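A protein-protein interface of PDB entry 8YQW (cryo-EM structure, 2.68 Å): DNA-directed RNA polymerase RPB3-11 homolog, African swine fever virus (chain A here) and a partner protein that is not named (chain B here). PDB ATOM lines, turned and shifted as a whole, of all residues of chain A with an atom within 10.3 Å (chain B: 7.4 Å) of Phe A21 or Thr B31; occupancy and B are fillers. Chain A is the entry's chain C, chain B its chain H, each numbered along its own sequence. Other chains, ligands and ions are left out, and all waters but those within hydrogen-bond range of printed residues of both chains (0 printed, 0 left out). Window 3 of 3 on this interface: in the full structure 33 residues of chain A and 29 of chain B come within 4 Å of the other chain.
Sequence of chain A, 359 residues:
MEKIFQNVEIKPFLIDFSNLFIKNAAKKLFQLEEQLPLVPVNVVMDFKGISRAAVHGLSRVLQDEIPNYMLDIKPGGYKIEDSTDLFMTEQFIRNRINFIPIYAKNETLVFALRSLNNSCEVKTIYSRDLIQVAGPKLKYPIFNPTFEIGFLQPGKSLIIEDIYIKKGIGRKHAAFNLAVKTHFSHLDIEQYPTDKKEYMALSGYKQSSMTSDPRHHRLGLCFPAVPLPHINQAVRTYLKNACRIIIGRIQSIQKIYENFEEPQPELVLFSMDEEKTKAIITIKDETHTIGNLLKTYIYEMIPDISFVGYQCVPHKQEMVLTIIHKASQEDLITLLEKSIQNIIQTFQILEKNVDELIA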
ATOM      1  N   ILE A  15      -2.370 -12.230 -16.489  1.00  0.00           N
ATOM      2  CA  ILE A  15      -2.017 -11.763 -17.823  1.00  0.00           C
ATOM      3  C   ILE A  15      -0.698 -11.009 -17.746  1.00  0.00           C
ATOM      4  O   ILE A  15      -0.520 -10.132 -16.894  1.00  0.00           O
ATOM      5  CB  ILE A  15      -3.129 -10.875 -18.404  1.00  0.00           C
ATOM      6  CG1 ILE A  15      -4.366 -11.712 -18.722  1.00  0.00           C
ATOM      7  CG2 ILE A  15      -2.647 -10.149 -19.645  1.00  0.00           C
ATOM      8  CD1 ILE A  15      -5.537 -10.899 -19.202  1.00  0.00           C
ATOM      9  N   ASP A  16       0.233 -11.355 -18.631  1.00  0.00           N
ATOM     10  CA  ASP A  16       1.524 -10.681 -18.711  1.00  0.00           C
ATOM     11  C   ASP A  16       1.383  -9.479 -19.635  1.00  0.00           C
ATOM     12  O   ASP A  16       1.265  -9.633 -20.854  1.00  0.00           O
ATOM     13  CB  ASP A  16       2.601 -11.641 -19.211  1.00  0.00           C
ATOM     14  CG  ASP A  16       4.002 -11.109 -19.000  1.00  0.00           C
ATOM     15  OD1 ASP A  16       4.145  -9.926 -18.629  1.00  0.00           O
ATOM     16  OD2 ASP A  16       4.965 -11.874 -19.211  1.00  0.00           O
ATOM     17  N   PHE A  17       1.398  -8.281 -19.057  1.00  0.00           N
ATOM     18  CA  PHE A  17       1.287  -7.051 -19.825  1.00  0.00           C
ATOM     19  C   PHE A  17       2.635  -6.525 -20.297  1.00  0.00           C
ATOM     20  O   PHE A  17       2.683  -5.469 -20.935  1.00  0.00           O
ATOM     21  CB  PHE A  17       0.562  -5.980 -19.005  1.00  0.00           C
ATOM     22  CG  PHE A  17      -0.918  -6.198 -18.904  1.00  0.00           C
ATOM     23  CD1 PHE A  17      -1.729  -6.052 -20.016  1.00  0.00           C
ATOM     24  CD2 PHE A  17      -1.499  -6.558 -17.704  1.00  0.00           C
ATOM     25  CE1 PHE A  17      -3.088  -6.257 -19.929  1.00  0.00           C
ATOM     26  CE2 PHE A  17      -2.858  -6.764 -17.611  1.00  0.00           C
ATOM     27  CZ  PHE A  17      -3.653  -6.613 -18.727  1.00  0.00           C
ATOM     28  N   SER A  18       3.726  -7.230 -19.999  1.00  0.00           N
ATOM     29  CA  SER A  18       5.018  -6.883 -20.576  1.00  0.00           C
ATOM     30  C   SER A  18       5.135  -7.320 -22.029  1.00  0.00           C
ATOM     31  O   SER A  18       6.108  -6.947 -22.693  1.00  0.00           O
ATOM     32  CB  SER A  18       6.150  -7.503 -19.758  1.00  0.00           C
ATOM     33  OG  SER A  18       6.193  -8.908 -19.927  1.00  0.00           O
ATOM     34  N   ASN A  19       4.182  -8.101 -22.530  1.00  0.00           N
ATOM     35  CA  ASN A  19       4.141  -8.459 -23.940  1.00  0.00           C
ATOM     36  C   ASN A  19       3.388  -7.374 -24.698  1.00  0.00           C
ATOM     37  O   ASN A  19       2.249  -7.043 -24.349  1.00  0.00           O
ATOM     38  CB  ASN A  19       3.476  -9.821 -24.128  1.00  0.00           C
ATOM     39  CG  ASN A  19       3.753 -10.422 -25.490  1.00  0.00           C
ATOM     40  OD1 ASN A  19       4.404  -9.807 -26.332  1.00  0.00           O
ATOM     41  ND2 ASN A  19       3.265 -11.633 -25.712  1.00  0.00           N
ATOM     42  N   LEU A  20       4.024  -6.818 -25.730  1.00  0.00           N
ATOM     43  CA  LEU A  20       3.452  -5.668 -26.421  1.00  0.00           C
ATOM     44  C   LEU A  20       2.191  -6.038 -27.190  1.00  0.00           C
ATOM     45  O   LEU A  20       1.236  -5.257 -27.227  1.00  0.00           O
ATOM     46  CB  LEU A  20       4.490  -5.050 -27.355  1.00  0.00           C
ATOM     47  CG  LEU A  20       5.568  -4.207 -26.672  1.00  0.00           C
ATOM     48  CD1 LEU A  20       6.271  -3.318 -27.684  1.00  0.00           C
ATOM     49  CD2 LEU A  20       4.968  -3.376 -25.544  1.00  0.00           C
ATOM     50  N   PHE A  21       2.168  -7.212 -27.823  1.00  0.00           N
ATOM     51  CA  PHE A  21       0.988  -7.611 -28.582  1.00  0.00           C
ATOM     52  C   PHE A  21      -0.218  -7.786 -27.667  1.00  0.00           C
ATOM     53  O   PHE A  21      -1.313  -7.291 -27.960  1.00  0.00           O
ATOM     54  CB  PHE A  21       1.268  -8.899 -29.354  1.00  0.00           C
ATOM     55  CG  PHE A  21       2.312  -8.751 -30.418  1.00  0.00           C
ATOM     56  CD1 PHE A  21       2.043  -8.042 -31.572  1.00  0.00           C
ATOM     57  CD2 PHE A  21       3.560  -9.324 -30.266  1.00  0.00           C
ATOM     58  CE1 PHE A  21       3.000  -7.903 -32.552  1.00  0.00           C
ATOM     59  CE2 PHE A  21       4.520  -9.188 -31.245  1.00  0.00           C
ATOM     60  CZ  PHE A  21       4.239  -8.477 -32.389  1.00  0.00           C
ATOM     61  N   ILE A  22      -0.028  -8.483 -26.545  1.00  0.00           N
ATOM     62  CA  ILE A  22      -1.121  -8.694 -25.602  1.00  0.00           C
ATOM     63  C   ILE A  22      -1.570  -7.370 -25.002  1.00  0.00           C
ATOM     64  O   ILE A  22      -2.770  -7.105 -24.870  1.00  0.00           O
ATOM     65  CB  ILE A  22      -0.700  -9.698 -24.514  1.00  0.00           C
ATOM     66  CG1 ILE A  22      -0.440 -11.071 -25.132  1.00  0.00           C
ATOM     67  CG2 ILE A  22      -1.760  -9.788 -23.431  1.00  0.00           C
ATOM     68  CD1 ILE A  22      -1.596 -11.598 -25.941  1.00  0.00           C
ATOM     69  N   LYS A  23      -0.612  -6.516 -24.636  1.00  0.00           N
ATOM     70  CA  LYS A  23      -0.943  -5.215 -24.064  1.00  0.00           C
ATOM     71  C   LYS A  23      -1.766  -4.379 -25.036  1.00  0.00           C
ATOM     72  O   LYS A  23      -2.799  -3.807 -24.665  1.00  0.00           O
ATOM     73  CB  LYS A  23       0.344  -4.486 -23.679  1.00  0.00           C
ATOM     74  CG  LYS A  23       0.145  -3.090 -23.131  1.00  0.00           C
ATOM     75  CD  LYS A  23       1.475  -2.465 -22.749  1.00  0.00           C
ATOM     76  CE  LYS A  23       1.310  -1.000 -22.382  1.00  0.00           C
ATOM     77  NZ  LYS A  23       0.528  -0.825 -21.128  1.00  0.00           N
ATOM     78  N   ASN A  24      -1.331  -4.312 -26.296  1.00  0.00           N
ATOM     79  CA  ASN A  24      -2.032  -3.497 -27.280  1.00  0.00           C
ATOM     80  C   ASN A  24      -3.412  -4.061 -27.589  1.00  0.00           C
ATOM     81  O   ASN A  24      -4.381  -3.305 -27.704  1.00  0.00           O
ATOM     82  CB  ASN A  24      -1.197  -3.379 -28.554  1.00  0.00           C
ATOM     83  CG  ASN A  24       0.079  -2.589 -28.342  1.00  0.00           C
ATOM     84  OD1 ASN A  24       0.121  -1.657 -27.537  1.00  0.00           O
ATOM     85  ND2 ASN A  24       1.127  -2.954 -29.067  1.00  0.00           N
ATOM     86  N   ALA A  25      -3.524  -5.386 -27.723  1.00  0.00           N
ATOM     87  CA  ALA A  25      -4.825  -5.984 -27.999  1.00  0.00           C
ATOM     88  C   ALA A  25      -5.789  -5.765 -26.842  1.00  0.00           C
ATOM     89  O   ALA A  25      -6.963  -5.442 -27.056  1.00  0.00           O
ATOM     90  CB  ALA A  25      -4.665  -7.474 -28.291  1.00  0.00           C
ATOM     91  N   ALA A  26      -5.311  -5.927 -25.607  1.00  0.00           N
ATOM     92  CA  ALA A  26      -6.173  -5.737 -24.449  1.00  0.00           C
ATOM     93  C   ALA A  26      -6.596  -4.283 -24.306  1.00  0.00           C
ATOM     94  O   ALA A  26      -7.732  -4.002 -23.908  1.00  0.00           O
ATOM     95  CB  ALA A  26      -5.461  -6.218 -23.185  1.00  0.00           C
ATOM     96  N   LYS A  27      -5.700  -3.343 -24.614  1.00  0.00           N
ATOM     97  CA  LYS A  27      -6.061  -1.935 -24.504  1.00  0.00           C
ATOM     98  C   LYS A  27      -7.033  -1.522 -25.603  1.00  0.00           C
ATOM     99  O   LYS A  27      -7.965  -0.751 -25.355  1.00  0.00           O
ATOM    100  CB  LYS A  27      -4.808  -1.063 -24.537  1.00  0.00           C
ATOM    101  CG  LYS A  27      -5.084   0.420 -24.363  1.00  0.00           C
ATOM    102  CD  LYS A  27      -3.797   1.224 -24.327  1.00  0.00           C
ATOM    103  CE  LYS A  27      -4.078   2.718 -24.379  1.00  0.00           C
ATOM    104  NZ  LYS A  27      -4.784   3.203 -23.162  1.00  0.00           N
ATOM    105  N   LYS A  28      -6.835  -2.023 -26.824  1.00  0.00           N
ATOM    106  CA  LYS A  28      -7.702  -1.627 -27.927  1.00  0.00           C
ATOM    107  C   LYS A  28      -9.069  -2.295 -27.862  1.00  0.00           C
ATOM    108  O   LYS A  28     -10.064  -1.691 -28.278  1.00  0.00           O
ATOM    109  CB  LYS A  28      -7.029  -1.945 -29.263  1.00  0.00           C
ATOM    110  CG  LYS A  28      -7.490  -1.058 -30.406  1.00  0.00           C
ATOM    111  CD  LYS A  28      -7.113  -1.649 -31.754  1.00  0.00           C
ATOM    112  CE  LYS A  28      -7.378  -0.661 -32.875  1.00  0.00           C
ATOM    113  NZ  LYS A  28      -6.763   0.667 -32.599  1.00  0.00           N
ATOM    114  N   LEU A  29      -9.148  -3.526 -27.355  1.00  0.00           N
ATOM    115  CA  LEU A  29     -10.423  -4.233 -27.325  1.00  0.00           C
ATOM    116  C   LEU A  29     -11.295  -3.779 -26.160  1.00  0.00           C
ATOM    117  O   LEU A  29     -12.400  -3.264 -26.361  1.00  0.00           O
ATOM    118  CB  LEU A  29     -10.183  -5.743 -27.259  1.00  0.00           C
ATOM    119  CG  LEU A  29      -9.894  -6.453 -28.579  1.00  0.00           C
ATOM    120  CD1 LEU A  29      -9.294  -7.815 -28.326  1.00  0.00           C
ATOM    121  CD2 LEU A  29     -11.168  -6.586 -29.388  1.00  0.00           C
ATOM    122  N   LEU A  32      -8.426  -2.502 -21.402  1.00  0.00           N
ATOM    123  CA  LEU A  32      -7.972  -3.284 -20.260  1.00  0.00           C
ATOM    124  C   LEU A  32      -6.521  -2.941 -19.953  1.00  0.00           C
ATOM    125  O   LEU A  32      -5.646  -3.090 -20.813  1.00  0.00           O
ATOM    126  CB  LEU A  32      -8.121  -4.779 -20.537  1.00  0.00           C
ATOM    127  CG  LEU A  32      -7.837  -5.723 -19.370  1.00  0.00           C
ATOM    128  CD1 LEU A  32      -8.842  -5.503 -18.258  1.00  0.00           C
ATOM    129  CD2 LEU A  32      -7.862  -7.166 -19.837  1.00  0.00           C
ATOM    130  N   ILE B  20      -8.744 -11.209 -27.167  1.00  0.00           N
ATOM    131  CA  ILE B  20      -7.398 -10.644 -27.130  1.00  0.00           C
ATOM    132  C   ILE B  20      -6.452 -11.496 -27.965  1.00  0.00           C
ATOM    133  O   ILE B  20      -5.780 -10.995 -28.877  1.00  0.00           O
ATOM    134  CB  ILE B  20      -6.911 -10.519 -25.676  1.00  0.00           C
ATOM    135  CG1 ILE B  20      -7.894  -9.687 -24.855  1.00  0.00           C
ATOM    136  CG2 ILE B  20      -5.526  -9.910 -25.626  1.00  0.00           C
ATOM    137  CD1 ILE B  20      -7.674  -9.786 -23.368  1.00  0.00           C
ATOM    138  N   LYS B  23      -6.720 -10.662 -31.699  1.00  0.00           N
ATOM    139  CA  LYS B  23      -6.109  -9.450 -32.232  1.00  0.00           C
ATOM    140  C   LYS B  23      -4.593  -9.552 -32.198  1.00  0.00           C
ATOM    141  O   LYS B  23      -3.927  -9.415 -33.233  1.00  0.00           O
ATOM    142  CB  LYS B  23      -6.592  -8.233 -31.445  1.00  0.00           C
ATOM    143  CG  LYS B  23      -6.039  -6.916 -31.947  1.00  0.00           C
ATOM    144  CD  LYS B  23      -6.684  -5.740 -31.238  1.00  0.00           C
ATOM    145  CE  LYS B  23      -8.102  -5.517 -31.730  1.00  0.00           C
ATOM    146  NZ  LYS B  23      -8.132  -5.067 -33.148  1.00  0.00           N
ATOM    147  N   ALA B  24      -4.042  -9.873 -31.027  1.00  0.00           N
ATOM    148  CA  ALA B  24      -2.599 -10.016 -30.888  1.00  0.00           C
ATOM    149  C   ALA B  24      -2.040 -10.949 -31.948  1.00  0.00           C
ATOM    150  O   ALA B  24      -1.059 -10.617 -32.624  1.00  0.00           O
ATOM    151  CB  ALA B  24      -2.257 -10.522 -29.489  1.00  0.00           C
ATOM    152  N   ARG B  25      -2.691 -12.100 -32.151  1.00  0.00           N
ATOM    153  CA  ARG B  25      -2.169 -13.063 -33.114  1.00  0.00           C
ATOM    154  C   ARG B  25      -2.002 -12.411 -34.475  1.00  0.00           C
ATOM    155  O   ARG B  25      -0.926 -12.485 -35.083  1.00  0.00           O
ATOM    156  CB  ARG B  25      -3.083 -14.283 -33.214  1.00  0.00           C
ATOM    157  CG  ARG B  25      -2.692 -15.231 -34.336  1.00  0.00           C
ATOM    158  CD  ARG B  25      -3.398 -16.564 -34.236  1.00  0.00           C
ATOM    159  NE  ARG B  25      -4.846 -16.437 -34.329  1.00  0.00           N
ATOM    160  CZ  ARG B  25      -5.685 -17.463 -34.319  1.00  0.00           C
ATOM    161  NH1 ARG B  25      -5.251 -18.708 -34.233  1.00  0.00           N
ATOM    162  NH2 ARG B  25      -6.991 -17.233 -34.401  1.00  0.00           N
ATOM    163  N   THR B  26      -3.033 -11.697 -34.931  1.00  0.00           N
ATOM    164  CA  THR B  26      -2.946 -11.046 -36.232  1.00  0.00           C
ATOM    165  C   THR B  26      -1.752 -10.107 -36.276  1.00  0.00           C
ATOM    166  O   THR B  26      -0.928 -10.178 -37.197  1.00  0.00           O
ATOM    167  CB  THR B  26      -4.241 -10.296 -36.534  1.00  0.00           C
ATOM    168  OG1 THR B  26      -5.342 -11.210 -36.485  1.00  0.00           O
ATOM    169  CG2 THR B  26      -4.179  -9.679 -37.915  1.00  0.00           C
ATOM    170  N   GLU B  27      -1.594  -9.280 -35.239  1.00  0.00           N
ATOM    171  CA  GLU B  27      -0.459  -8.366 -35.203  1.00  0.00           C
ATOM    172  C   GLU B  27       0.845  -9.138 -35.324  1.00  0.00           C
ATOM    173  O   GLU B  27       1.710  -8.795 -36.141  1.00  0.00           O
ATOM    174  CB  GLU B  27      -0.482  -7.543 -33.916  1.00  0.00           C
ATOM    175  CG  GLU B  27      -1.857  -7.049 -33.504  1.00  0.00           C
ATOM    176  CD  GLU B  27      -1.836  -6.265 -32.201  1.00  0.00           C
ATOM    177  OE1 GLU B  27      -0.754  -6.147 -31.587  1.00  0.00           O
ATOM    178  OE2 GLU B  27      -2.904  -5.770 -31.784  1.00  0.00           O
ATOM    179  N   TYR B  28       0.970 -10.233 -34.570  1.00  0.00           N
ATOM    180  CA  TYR B  28       2.195 -11.017 -34.628  1.00  0.00           C
ATOM    181  C   TYR B  28       2.449 -11.507 -36.044  1.00  0.00           C
ATOM    182  O   TYR B  28       3.569 -11.394 -36.558  1.00  0.00           O
ATOM    183  CB  TYR B  28       2.113 -12.186 -33.648  1.00  0.00           C
ATOM    184  CG  TYR B  28       3.305 -13.113 -33.685  1.00  0.00           C
ATOM    185  CD1 TYR B  28       4.477 -12.796 -33.019  1.00  0.00           C
ATOM    186  CD2 TYR B  28       3.253 -14.314 -34.379  1.00  0.00           C
ATOM    187  CE1 TYR B  28       5.564 -13.641 -33.049  1.00  0.00           C
ATOM    188  CE2 TYR B  28       4.334 -15.163 -34.415  1.00  0.00           C
ATOM    189  CZ  TYR B  28       5.487 -14.824 -33.749  1.00  0.00           C
ATOM    190  OH  TYR B  28       6.568 -15.675 -33.784  1.00  0.00           O
ATOM    191  N   ILE B  29       1.402 -11.990 -36.717  1.00  0.00           N
ATOM    192  CA  ILE B  29       1.583 -12.500 -38.070  1.00  0.00           C
ATOM    193  C   ILE B  29       2.021 -11.376 -38.997  1.00  0.00           C
ATOM    194  O   ILE B  29       2.869 -11.573 -39.876  1.00  0.00           O
ATOM    195  CB  ILE B  29       0.296 -13.188 -38.560  1.00  0.00           C
ATOM    196  CG1 ILE B  29       0.062 -14.478 -37.773  1.00  0.00           C
ATOM    197  CG2 ILE B  29       0.382 -13.495 -40.044  1.00  0.00           C
ATOM    198  CD1 ILE B  29      -1.278 -15.114 -38.026  1.00  0.00           C
ATOM    199  N   LYS B  30       1.495 -10.168 -38.777  1.00  0.00           N
ATOM    200  CA  LYS B  30       1.873  -9.044 -39.626  1.00  0.00           C
ATOM    201  C   LYS B  30       3.363  -8.761 -39.537  1.00  0.00           C
ATOM    202  O   LYS B  30       3.947  -8.210 -40.476  1.00  0.00           O
ATOM    203  CB  LYS B  30       1.068  -7.804 -39.248  1.00  0.00           C
ATOM    204  CG  LYS B  30      -0.321  -7.764 -39.852  1.00  0.00           C
ATOM    205  CD  LYS B  30      -1.009  -6.447 -39.553  1.00  0.00           C
ATOM    206  CE  LYS B  30      -2.517  -6.607 -39.540  1.00  0.00           C
ATOM    207  NZ  LYS B  30      -3.169  -5.665 -38.589  1.00  0.00           N
ATOM    208  N   THR B  31       3.998  -9.134 -38.425  1.00  0.00           N
ATOM    209  CA  THR B  31       5.438  -8.946 -38.314  1.00  0.00           C
ATOM    210  C   THR B  31       6.194  -9.990 -39.128  1.00  0.00           C
ATOM    211  O   THR B  31       7.210  -9.678 -39.759  1.00  0.00           O
ATOM    212  CB  THR B  31       5.858  -8.991 -36.845  1.00  0.00           C
ATOM    213  OG1 THR B  31       5.273  -7.884 -36.148  1.00  0.00           O
ATOM    214  CG2 THR B  31       7.366  -8.918 -36.711  1.00  0.00           C
ATOM    215  N   LYS B  32       5.700 -11.225 -39.149  1.00  0.00           N
ATOM    216  CA  LYS B  32       6.418 -12.339 -39.750  1.00  0.00           C
ATOM    217  C   LYS B  32       5.991 -12.632 -41.180  1.00  0.00           C
ATOM    218  O   LYS B  32       6.624 -13.463 -41.838  1.00  0.00           O
ATOM    219  CB  LYS B  32       6.233 -13.603 -38.903  1.00  0.00           C
ATOM    220  CG  LYS B  32       6.681 -13.476 -37.461  1.00  0.00           C
ATOM    221  CD  LYS B  32       8.189 -13.416 -37.351  1.00  0.00           C
ATOM    222  CE  LYS B  32       8.634 -13.455 -35.899  1.00  0.00           C
ATOM    223  NZ  LYS B  32       8.286 -12.201 -35.177  1.00  0.00           N
ATOM    224  N   MET B  33       4.943 -11.977 -41.677  1.00  0.00           N
ATOM    225  CA  MET B  33       4.315 -12.386 -42.928  1.00  0.00           C
ATOM    226  C   MET B  33       5.266 -12.293 -44.116  1.00  0.00           C
ATOM    227  O   MET B  33       5.702 -13.323 -44.640  1.00  0.00           O
ATOM    228  CB  MET B  33       3.067 -11.530 -43.156  1.00  0.00           C
ATOM    229  CG  MET B  33       2.360 -11.731 -44.471  1.00  0.00           C
ATOM    230  SD  MET B  33       0.806 -10.823 -44.486  1.00  0.00           S
ATOM    231  CE  MET B  33       1.399  -9.143 -44.326  1.00  0.00           C
ATOM    232  N   GLY B  34       5.594 -11.084 -44.559  1.00  0.00           N
ATOM    233  CA  GLY B  34       6.754 -10.895 -45.409  1.00  0.00           C
ATOM    234  C   GLY B  34       6.473 -11.097 -46.883  1.00  0.00           C
ATOM    235  O   GLY B  34       6.405 -12.244 -47.331  1.00  0.00           O
ATOM    236  N   LEU B  54       3.192 -15.934 -26.913  1.00  0.00           N
ATOM    237  CA  LEU B  54       1.993 -15.104 -26.937  1.00  0.00           C
ATOM    238  C   LEU B  54       0.894 -15.693 -26.064  1.00  0.00           C
ATOM    239  O   LEU B  54       0.238 -14.971 -25.307  1.00  0.00           O
ATOM    240  CB  LEU B  54       1.510 -14.944 -28.378  1.00  0.00           C
ATOM    241  CG  LEU B  54       0.760 -13.669 -28.751  1.00  0.00           C
ATOM    242  CD1 LEU B  54       1.646 -12.462 -28.544  1.00  0.00           C
ATOM    243  CD2 LEU B  54       0.303 -13.751 -30.191  1.00  0.00           C
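Hydrophobic or aromatic side chains of chain A within 4 Å of the printed part of chain B: Phe A21, Ile A22, Ala A25 and Leu A29. Of the 14 printed residues of chain B, 7 touch a printed residue of chain A. Hydrophobic or aromatic side chains of chain B that line the printed part of chain A: Ile B20, Ala B24 and Leu B54. Along chain B the printed residues that touch a printed residue of chain A span positions 20 to 54.
Thr B31 touches just one residue of chain A: Phe A21 (3.9 Å). Of chain A, only Phe A21 (3.7 Å), Ile A22 (3.8 Å) and Ala A25 (3.7 Å) come within 4 Å of Ala B24. Glu B27 touches one residue of chain A. Printed residues of chain B within 4 Å of Lys A28: Lys B23. Of the printed residues of chain B, Leu A29 touches Ile B20 (3.6 Å) and Lys B23 (3.7 Å). Of the printed residues of chain A, Leu B54 touches Asn A19, Phe A21 and Ile A22. Printed residues of chain B within 4 Å of Ala A25: Ile B20, Lys B23 and Ala B24. Thr B26 touches none of the printed residues of chain A. Lys A27 touches none of the printed residues of chain B. The nearest residue of chain B that does not touch Phe A21 is Ile B20 (5.5 Å). The nearest printed residue of chain A that does not touch Leu B54 is Leu A20 (6.6 Å).
O of Ala A26 lies within hydrogen-bond range of N of Leu A32, at 3.0 Å.
Phe A21 touches Glu B27. OG1 of Thr B31 touches CZ of Phe A21, 3.9 Å away. Phe A21 touches Leu B54 (CB to CD1, 3.7 Å). Ile A22 touches Ala B24. Ile A22 touches Leu B54. CG2 of Ile B20 touches CB of Ala A25, at 3.7 Å. CA of Ala A25 touches CD of Lys B23, 3.7 Å away. N of Ala B24 touches CB of Ala A25, at 3.7 Å. Lys B23 touches Lys A28 (NZ to CD, 3.8 Å). Leu A29 touches Ile B20.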
